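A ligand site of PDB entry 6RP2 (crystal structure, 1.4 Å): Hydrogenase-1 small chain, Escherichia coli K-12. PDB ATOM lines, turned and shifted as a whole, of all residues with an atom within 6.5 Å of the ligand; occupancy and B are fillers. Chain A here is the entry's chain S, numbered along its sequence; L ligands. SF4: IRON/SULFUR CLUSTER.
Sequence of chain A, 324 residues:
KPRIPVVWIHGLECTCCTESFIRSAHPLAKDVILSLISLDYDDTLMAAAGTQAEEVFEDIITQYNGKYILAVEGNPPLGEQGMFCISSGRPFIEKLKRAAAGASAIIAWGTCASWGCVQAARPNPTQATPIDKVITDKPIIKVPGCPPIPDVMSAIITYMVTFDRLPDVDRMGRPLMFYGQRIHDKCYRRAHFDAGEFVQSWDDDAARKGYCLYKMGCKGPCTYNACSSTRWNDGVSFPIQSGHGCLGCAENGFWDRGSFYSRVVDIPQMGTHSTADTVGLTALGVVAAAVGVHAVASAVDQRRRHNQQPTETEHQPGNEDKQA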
ATOM      1  N   ILE A 183      12.172 -25.829  16.991  1.00  0.00           N
ATOM      2  CA  ILE A 183      11.679 -25.802  15.590  1.00  0.00           C
ATOM      3  C   ILE A 183      12.297 -24.619  14.868  1.00  0.00           C
ATOM      4  O   ILE A 183      12.770 -24.745  13.734  1.00  0.00           O
ATOM      5  CB  ILE A 183      10.127 -25.674  15.610  1.00  0.00           C
ATOM      6  CG1 ILE A 183       9.452 -26.934  16.147  1.00  0.00           C
ATOM      7  CG2 ILE A 183       9.568 -25.282  14.262  1.00  0.00           C
ATOM      8  CD1 ILE A 183       9.777 -28.190  15.402  1.00  0.00           C
ATOM      9  N   HIS A 184      12.312 -23.445  15.485  1.00  0.00           N
ATOM     10  CA  HIS A 184      12.798 -22.183  14.900  1.00  0.00           C
ATOM     11  C   HIS A 184      14.314 -22.171  14.674  1.00  0.00           C
ATOM     12  O   HIS A 184      14.768 -21.335  13.907  1.00  0.00           O
ATOM     13  CB  HIS A 184      12.331 -21.070  15.854  1.00  0.00           C
ATOM     14  CG  HIS A 184      12.658 -19.662  15.566  1.00  0.00           C
ATOM     15  ND1 HIS A 184      12.039 -18.863  14.577  1.00  0.00           N
ATOM     16  CD2 HIS A 184      13.488 -18.850  16.252  1.00  0.00           C
ATOM     17  CE1 HIS A 184      12.529 -17.615  14.738  1.00  0.00           C
ATOM     18  NE2 HIS A 184      13.416 -17.586  15.699  1.00  0.00           N
ATOM     19  N   ASP A 185      15.052 -23.072  15.313  1.00  0.00           N
ATOM     20  CA  ASP A 185      16.509 -23.063  15.126  1.00  0.00           C
ATOM     21  C   ASP A 185      16.886 -24.000  13.969  1.00  0.00           C
ATOM     22  O   ASP A 185      18.109 -24.089  13.685  1.00  0.00           O
ATOM     23  CB  ASP A 185      17.204 -23.330  16.457  1.00  0.00           C
ATOM     24  CG  ASP A 185      17.133 -22.176  17.445  1.00  0.00           C
ATOM     25  OD1 ASP A 185      16.852 -21.024  17.047  1.00  0.00           O
ATOM     26  OD2 ASP A 185      17.317 -22.454  18.613  1.00  0.00           O
ATOM     27  N   CYS A 187      14.407 -24.028  11.117  1.00  0.00           N
ATOM     28  CA  CYS A 187      13.268 -23.717  10.218  1.00  0.00           C
ATOM     29  C   CYS A 187      13.786 -23.132   8.913  1.00  0.00           C
ATOM     30  O   CYS A 187      14.481 -22.115   8.908  1.00  0.00           O
ATOM     31  CB  CYS A 187      12.285 -22.789  10.901  1.00  0.00           C
ATOM     32  SG  CYS A 187      10.825 -22.470   9.890  1.00  0.00           S
ATOM     33  N   TYR A 188      13.299 -23.667   7.824  1.00  0.00           N
ATOM     34  CA  TYR A 188      13.695 -23.216   6.464  1.00  0.00           C
ATOM     35  C   TYR A 188      13.120 -21.827   6.156  1.00  0.00           C
ATOM     36  O   TYR A 188      13.562 -21.231   5.174  1.00  0.00           O
ATOM     37  CB  TYR A 188      13.319 -24.264   5.409  1.00  0.00           C
ATOM     38  CG  TYR A 188      11.903 -24.200   4.911  1.00  0.00           C
ATOM     39  CD1 TYR A 188      10.803 -24.320   5.758  1.00  0.00           C
ATOM     40  CD2 TYR A 188      11.629 -24.099   3.548  1.00  0.00           C
ATOM     41  CE1 TYR A 188       9.504 -24.253   5.265  1.00  0.00           C
ATOM     42  CE2 TYR A 188      10.336 -24.038   3.060  1.00  0.00           C
ATOM     43  CZ  TYR A 188       9.253 -24.102   3.926  1.00  0.00           C
ATOM     44  OH  TYR A 188       7.982 -23.988   3.433  1.00  0.00           O
ATOM     45  N   ARG A 189      12.231 -21.272   6.972  1.00  0.00           N
ATOM     46  CA  ARG A 189      11.747 -19.886   6.757  1.00  0.00           C
ATOM     47  C   ARG A 189      12.495 -18.906   7.648  1.00  0.00           C
ATOM     48  O   ARG A 189      12.121 -17.702   7.628  1.00  0.00           O
ATOM     49  CB  ARG A 189      10.236 -19.807   6.962  1.00  0.00           C
ATOM     50  CG  ARG A 189       9.433 -20.662   5.988  1.00  0.00           C
ATOM     51  CD  ARG A 189       7.946 -20.490   6.104  1.00  0.00           C
ATOM     52  NE  ARG A 189       7.255 -21.389   5.215  1.00  0.00           N
ATOM     53  CZ  ARG A 189       6.037 -21.238   4.720  1.00  0.00           C
ATOM     54  NH1 ARG A 189       5.324 -20.152   4.995  1.00  0.00           N
ATOM     55  NH2 ARG A 189       5.517 -22.150   3.920  1.00  0.00           N
ATOM     56  N   ARG A 190      13.541 -19.307   8.350  1.00  0.00           N
ATOM     57  CA  ARG A 190      14.270 -18.394   9.249  1.00  0.00           C
ATOM     58  C   ARG A 190      14.841 -17.219   8.464  1.00  0.00           C
ATOM     59  O   ARG A 190      14.907 -16.111   9.019  1.00  0.00           O
ATOM     60  CB  ARG A 190      15.360 -19.169   9.962  1.00  0.00           C
ATOM     61  CG  ARG A 190      16.027 -18.369  11.053  1.00  0.00           C
ATOM     62  CD  ARG A 190      15.066 -17.960  12.192  1.00  0.00           C
ATOM     63  NE  ARG A 190      15.976 -17.220  13.002  1.00  0.00           N
ATOM     64  CZ  ARG A 190      16.603 -17.668  14.076  1.00  0.00           C
ATOM     65  NH1 ARG A 190      16.342 -18.828  14.635  1.00  0.00           N
ATOM     66  NH2 ARG A 190      17.493 -16.887  14.622  1.00  0.00           N
ATOM     67  N   ALA A 191      15.273 -17.403   7.216  1.00  0.00           N
ATOM     68  CA  ALA A 191      15.780 -16.283   6.408  1.00  0.00           C
ATOM     69  C   ALA A 191      14.760 -15.162   6.428  1.00  0.00           C
ATOM     70  O   ALA A 191      15.130 -13.956   6.466  1.00  0.00           O
ATOM     71  CB  ALA A 191      16.040 -16.711   4.982  1.00  0.00           C
ATOM     72  N   HIS A 192      13.474 -15.496   6.256  1.00  0.00           N
ATOM     73  CA  HIS A 192      12.411 -14.474   6.174  1.00  0.00           C
ATOM     74  C   HIS A 192      12.218 -13.821   7.542  1.00  0.00           C
ATOM     75  O   HIS A 192      12.082 -12.582   7.623  1.00  0.00           O
ATOM     76  CB  HIS A 192      11.144 -15.114   5.644  1.00  0.00           C
ATOM     77  CG  HIS A 192      11.290 -15.695   4.272  1.00  0.00           C
ATOM     78  ND1 HIS A 192      11.758 -14.932   3.218  1.00  0.00           N
ATOM     79  CD2 HIS A 192      11.089 -16.947   3.819  1.00  0.00           C
ATOM     80  CE1 HIS A 192      11.785 -15.730   2.134  1.00  0.00           C
ATOM     81  NE2 HIS A 192      11.370 -16.992   2.478  1.00  0.00           N
ATOM     82  N   PHE A 193      12.195 -14.589   8.606  1.00  0.00           N
ATOM     83  CA  PHE A 193      12.132 -14.046   9.978  1.00  0.00           C
ATOM     84  C   PHE A 193      13.260 -13.030  10.185  1.00  0.00           C
ATOM     85  O   PHE A 193      12.979 -11.857  10.587  1.00  0.00           O
ATOM     86  CB  PHE A 193      12.249 -15.185  10.978  1.00  0.00           C
ATOM     87  CG  PHE A 193      12.279 -14.728  12.414  1.00  0.00           C
ATOM     88  CD1 PHE A 193      11.105 -14.589  13.120  1.00  0.00           C
ATOM     89  CD2 PHE A 193      13.477 -14.458  13.053  1.00  0.00           C
ATOM     90  CE1 PHE A 193      11.100 -14.194  14.448  1.00  0.00           C
ATOM     91  CE2 PHE A 193      13.476 -14.111  14.400  1.00  0.00           C
ATOM     92  CZ  PHE A 193      12.291 -13.942  15.079  1.00  0.00           C
ATOM     93  N   PHE A 198       7.235 -11.320   6.546  1.00  0.00           N
ATOM     94  CA  PHE A 198       6.205 -12.046   7.312  1.00  0.00           C
ATOM     95  C   PHE A 198       4.909 -12.112   6.520  1.00  0.00           C
ATOM     96  O   PHE A 198       4.495 -11.123   5.913  1.00  0.00           O
ATOM     97  CB  PHE A 198       5.947 -11.296   8.616  1.00  0.00           C
ATOM     98  CG  PHE A 198       7.136 -11.214   9.528  1.00  0.00           C
ATOM     99  CD1 PHE A 198       7.645 -12.342  10.130  1.00  0.00           C
ATOM    100  CD2 PHE A 198       7.702  -9.984   9.852  1.00  0.00           C
ATOM    101  CE1 PHE A 198       8.724 -12.255  10.987  1.00  0.00           C
ATOM    102  CE2 PHE A 198       8.732  -9.893  10.745  1.00  0.00           C
ATOM    103  CZ  PHE A 198       9.253 -11.023  11.317  1.00  0.00           C
ATOM    104  N   TYR A 211       6.842 -16.912   3.193  1.00  0.00           N
ATOM    105  CA  TYR A 211       7.431 -16.051   4.233  1.00  0.00           C
ATOM    106  C   TYR A 211       7.095 -16.606   5.623  1.00  0.00           C
ATOM    107  O   TYR A 211       6.298 -17.539   5.826  1.00  0.00           O
ATOM    108  CB  TYR A 211       6.954 -14.613   4.026  1.00  0.00           C
ATOM    109  CG  TYR A 211       7.664 -13.851   2.919  1.00  0.00           C
ATOM    110  CD1 TYR A 211       8.530 -14.448   2.036  1.00  0.00           C
ATOM    111  CD2 TYR A 211       7.455 -12.470   2.799  1.00  0.00           C
ATOM    112  CE1 TYR A 211       9.169 -13.725   1.028  1.00  0.00           C
ATOM    113  CE2 TYR A 211       8.115 -11.745   1.840  1.00  0.00           C
ATOM    114  CZ  TYR A 211       8.923 -12.384   0.926  1.00  0.00           C
ATOM    115  OH  TYR A 211       9.555 -11.645  -0.060  1.00  0.00           O
ATOM    116  N   CYS A 212       7.791 -16.046   6.612  1.00  0.00           N
ATOM    117  CA  CYS A 212       7.756 -16.490   8.011  1.00  0.00           C
ATOM    118  C   CYS A 212       6.353 -16.266   8.584  1.00  0.00           C
ATOM    119  O   CYS A 212       5.695 -15.269   8.244  1.00  0.00           O
ATOM    120  CB  CYS A 212       8.855 -15.790   8.798  1.00  0.00           C
ATOM    121  SG  CYS A 212       8.718 -16.008  10.596  1.00  0.00           S
ATOM    122  N   LEU A 213       5.945 -17.160   9.454  1.00  0.00           N
ATOM    123  CA  LEU A 213       4.581 -17.236  10.062  1.00  0.00           C
ATOM    124  C   LEU A 213       4.563 -16.667  11.465  1.00  0.00           C
ATOM    125  O   LEU A 213       3.547 -16.794  12.171  1.00  0.00           O
ATOM    126  CB  LEU A 213       4.075 -18.684   9.982  1.00  0.00           C
ATOM    127  CG  LEU A 213       3.956 -19.189   8.555  1.00  0.00           C
ATOM    128  CD1 LEU A 213       3.673 -20.688   8.543  1.00  0.00           C
ATOM    129  CD2 LEU A 213       2.856 -18.486   7.802  1.00  0.00           C
ATOM    130  N   TYR A 214       5.627 -15.998  11.902  1.00  0.00           N
ATOM    131  CA  TYR A 214       5.704 -15.434  13.273  1.00  0.00           C
ATOM    132  C   TYR A 214       4.503 -14.530  13.591  1.00  0.00           C
ATOM    133  O   TYR A 214       3.882 -14.651  14.656  1.00  0.00           O
ATOM    134  CB  TYR A 214       6.998 -14.625  13.376  1.00  0.00           C
ATOM    135  CG  TYR A 214       7.074 -13.802  14.636  1.00  0.00           C
ATOM    136  CD1 TYR A 214       7.283 -14.415  15.852  1.00  0.00           C
ATOM    137  CD2 TYR A 214       6.895 -12.433  14.560  1.00  0.00           C
ATOM    138  CE1 TYR A 214       7.375 -13.661  17.014  1.00  0.00           C
ATOM    139  CE2 TYR A 214       6.982 -11.673  15.716  1.00  0.00           C
ATOM    140  CZ  TYR A 214       7.183 -12.303  16.925  1.00  0.00           C
ATOM    141  OH  TYR A 214       7.246 -11.501  18.042  1.00  0.00           O
ATOM    142  N   LYS A 215       4.160 -13.621  12.685  1.00  0.00           N
ATOM    143  CA  LYS A 215       3.038 -12.662  12.941  1.00  0.00           C
ATOM    144  C   LYS A 215       1.680 -13.350  12.847  1.00  0.00           C
ATOM    145  O   LYS A 215       0.645 -12.793  13.300  1.00  0.00           O
ATOM    146  CB  LYS A 215       3.125 -11.456  12.006  1.00  0.00           C
ATOM    147  CG  LYS A 215       4.314 -10.582  12.273  1.00  0.00           C
ATOM    148  CD  LYS A 215       4.243  -9.262  11.551  1.00  0.00           C
ATOM    149  CE  LYS A 215       5.398  -8.389  11.954  1.00  0.00           C
ATOM    150  NZ  LYS A 215       5.362  -7.110  11.209  1.00  0.00           N
ATOM    151  N   CYS A 218       3.045 -18.231  14.948  1.00  0.00           N
ATOM    152  CA  CYS A 218       3.914 -19.432  14.987  1.00  0.00           C
ATOM    153  C   CYS A 218       4.618 -19.535  16.345  1.00  0.00           C
ATOM    154  O   CYS A 218       5.303 -18.597  16.785  1.00  0.00           O
ATOM    155  CB  CYS A 218       4.976 -19.336  13.901  1.00  0.00           C
ATOM    156  SG  CYS A 218       6.011 -20.812  13.805  1.00  0.00           S
ATOM    157  N   LYS A 219       4.527 -20.700  16.949  1.00  0.00           N
ATOM    158  CA  LYS A 219       5.165 -20.986  18.250  1.00  0.00           C
ATOM    159  C   LYS A 219       6.480 -21.728  18.108  1.00  0.00           C
ATOM    160  O   LYS A 219       7.076 -22.162  19.108  1.00  0.00           O
ATOM    161  CB  LYS A 219       4.167 -21.702  19.164  1.00  0.00           C
ATOM    162  CG  LYS A 219       2.927 -20.854  19.484  1.00  0.00           C
ATOM    163  CD  LYS A 219       3.253 -19.395  19.839  1.00  0.00           C
ATOM    164  CE  LYS A 219       2.143 -18.491  20.320  1.00  0.00           C
ATOM    165  NZ  LYS A 219       0.933 -18.529  19.487  1.00  0.00           N
ATOM    166  N   GLY A 220       6.999 -21.801  16.895  1.00  0.00           N
ATOM    167  CA  GLY A 220       8.302 -22.422  16.641  1.00  0.00           C
ATOM    168  C   GLY A 220       9.425 -21.906  17.536  1.00  0.00           C
ATOM    169  O   GLY A 220      10.306 -22.679  17.950  1.00  0.00           O
ATOM    170  N   PRO A 221       9.467 -20.588  17.855  1.00  0.00           N
ATOM    171  CA  PRO A 221      10.548 -20.054  18.707  1.00  0.00           C
ATOM    172  C   PRO A 221      10.568 -20.626  20.117  1.00  0.00           C
ATOM    173  O   PRO A 221      11.609 -20.458  20.766  1.00  0.00           O
ATOM    174  CB  PRO A 221      10.253 -18.559  18.729  1.00  0.00           C
ATOM    175  CG  PRO A 221       9.637 -18.308  17.407  1.00  0.00           C
ATOM    176  CD  PRO A 221       8.695 -19.498  17.257  1.00  0.00           C
ATOM    177  N   PHE A 238       5.731 -30.348   7.011  1.00  0.00           N
ATOM    178  CA  PHE A 238       5.469 -30.128   8.446  1.00  0.00           C
ATOM    179  C   PHE A 238       4.529 -28.937   8.520  1.00  0.00           C
ATOM    180  O   PHE A 238       4.288 -28.262   7.529  1.00  0.00           O
ATOM    181  CB  PHE A 238       6.774 -29.987   9.249  1.00  0.00           C
ATOM    182  CG  PHE A 238       7.572 -28.702   9.139  1.00  0.00           C
ATOM    183  CD1 PHE A 238       8.258 -28.352   7.988  1.00  0.00           C
ATOM    184  CD2 PHE A 238       7.735 -27.900  10.259  1.00  0.00           C
ATOM    185  CE1 PHE A 238       9.047 -27.212   7.937  1.00  0.00           C
ATOM    186  CE2 PHE A 238       8.514 -26.762  10.199  1.00  0.00           C
ATOM    187  CZ  PHE A 238       9.157 -26.421   9.032  1.00  0.00           C
ATOM    188  N   ILE A 240       4.553 -25.739   9.321  1.00  0.00           N
ATOM    189  CA  ILE A 240       5.014 -24.450   8.753  1.00  0.00           C
ATOM    190  C   ILE A 240       5.201 -24.576   7.244  1.00  0.00           C
ATOM    191  O   ILE A 240       4.850 -23.646   6.501  1.00  0.00           O
ATOM    192  CB  ILE A 240       6.297 -24.034   9.480  1.00  0.00           C
ATOM    193  CG1 ILE A 240       5.994 -23.501  10.879  1.00  0.00           C
ATOM    194  CG2 ILE A 240       7.095 -23.010   8.667  1.00  0.00           C
ATOM    195  CD1 ILE A 240       7.119 -23.756  11.877  1.00  0.00           C
ATOM    196  N   GLY A 245       1.417 -21.715  11.197  1.00  0.00           N
ATOM    197  CA  GLY A 245       2.432 -21.639  12.261  1.00  0.00           C
ATOM    198  C   GLY A 245       2.393 -22.884  13.130  1.00  0.00           C
ATOM    199  O   GLY A 245       1.328 -23.503  13.335  1.00  0.00           O
ATOM    200  N   CYS A 246       3.515 -23.225  13.710  1.00  0.00           N
ATOM    201  CA  CYS A 246       3.597 -24.209  14.822  1.00  0.00           C
ATOM    202  C   CYS A 246       2.623 -23.787  15.919  1.00  0.00           C
ATOM    203  O   CYS A 246       2.549 -22.583  16.262  1.00  0.00           O
ATOM    204  CB  CYS A 246       5.044 -24.286  15.294  1.00  0.00           C
ATOM    205  SG  CYS A 246       5.383 -25.333  16.737  1.00  0.00           S
HETATM  206 FE1  SF4 L   1       9.159 -18.118  11.256  1.00  0.00          FE
HETATM  207 FE2  SF4 L   1       7.932 -20.022  12.805  1.00  0.00          FE
HETATM  208 FE3  SF4 L   1      10.530 -19.301  13.291  1.00  0.00          FE
HETATM  209 FE4  SF4 L   1       9.934 -20.727  11.064  1.00  0.00          FE
HETATM  210  S1  SF4 L   1       9.702 -21.417  13.258  1.00  0.00           S
HETATM  211  S2  SF4 L   1      11.285 -18.915  11.154  1.00  0.00           S
HETATM  212  S3  SF4 L   1       7.903 -19.851  10.466  1.00  0.00           S
HETATM  213  S4  SF4 L   1       8.653 -18.009  13.526  1.00  0.00           S
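An iron atom (FE3) of the ligand is bound by a ring nitrogen (ND1) of His 184 (2.0 Å).
An iron atom (FE1) of the ligand is bound by the side-chain sulfur of Cys 212 (2.3 Å).
An iron atom (FE4) of the ligand is bound by the side-chain sulfur (SG) of Cys 187 (2.3 Å).
The side-chain sulfur (SG) of Cys 218 is bound to an iron atom (FE2) of the ligand, 2.3 Å away.
A sulfur (S3) of the ligand sits close to the backbone NH (N) of Leu 213, 3.5 Å away.
N of Arg 190 sits close to S2 of the ligand (3.6 Å).
The guanidinium group (NH1) of Arg 190 is in hydrogen-bond range of the backbone carbonyl oxygen (O) of His 184, 3.0 Å away.
N of Tyr 214 lies close to SG of Cys 212 (3.4 Å).
N of Arg 189 sits close to SG of Cys 187 (3.5 Å).
The backbone NH of Cys 218 lies within hydrogen-bond range of the backbone carbonyl oxygen of Leu 213, 3.2 Å away.
The side-chain sulfur (SG) of Cys 218 lies close to the backbone NH (N) of Gly 220 (3.4 Å).
NH1 of Arg 190 is in salt-bridge range of OD1 of Asp 185, at 3.3 Å.
The guanidinium group of Arg 189 sits at hydrogen-bond distance from the backbone carbonyl oxygen of Ile 240 (3.1 Å).
OH of Tyr 188 is in hydrogen-bond range of NH2 of Arg 189.
Residues that only touch the ligand: Arg 189 (3.7 Å), Ile 240 (3.7 Å), Tyr 214 (3.8 Å), Gly 220 (3.8 Å), Phe 193 (3.9 Å) and Ile 183 (3.996 Å).
12 residues have an atom within 4 Å of the ligand: Ile 183, His 184, Cys 187, Arg 189, Arg 190, Phe 193, Cys 212, Leu 213, Tyr 214, Cys 218, Gly 220 and Ile 240.
Along chain A the residues within 4 Å of the ligand span positions 183 to 240.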
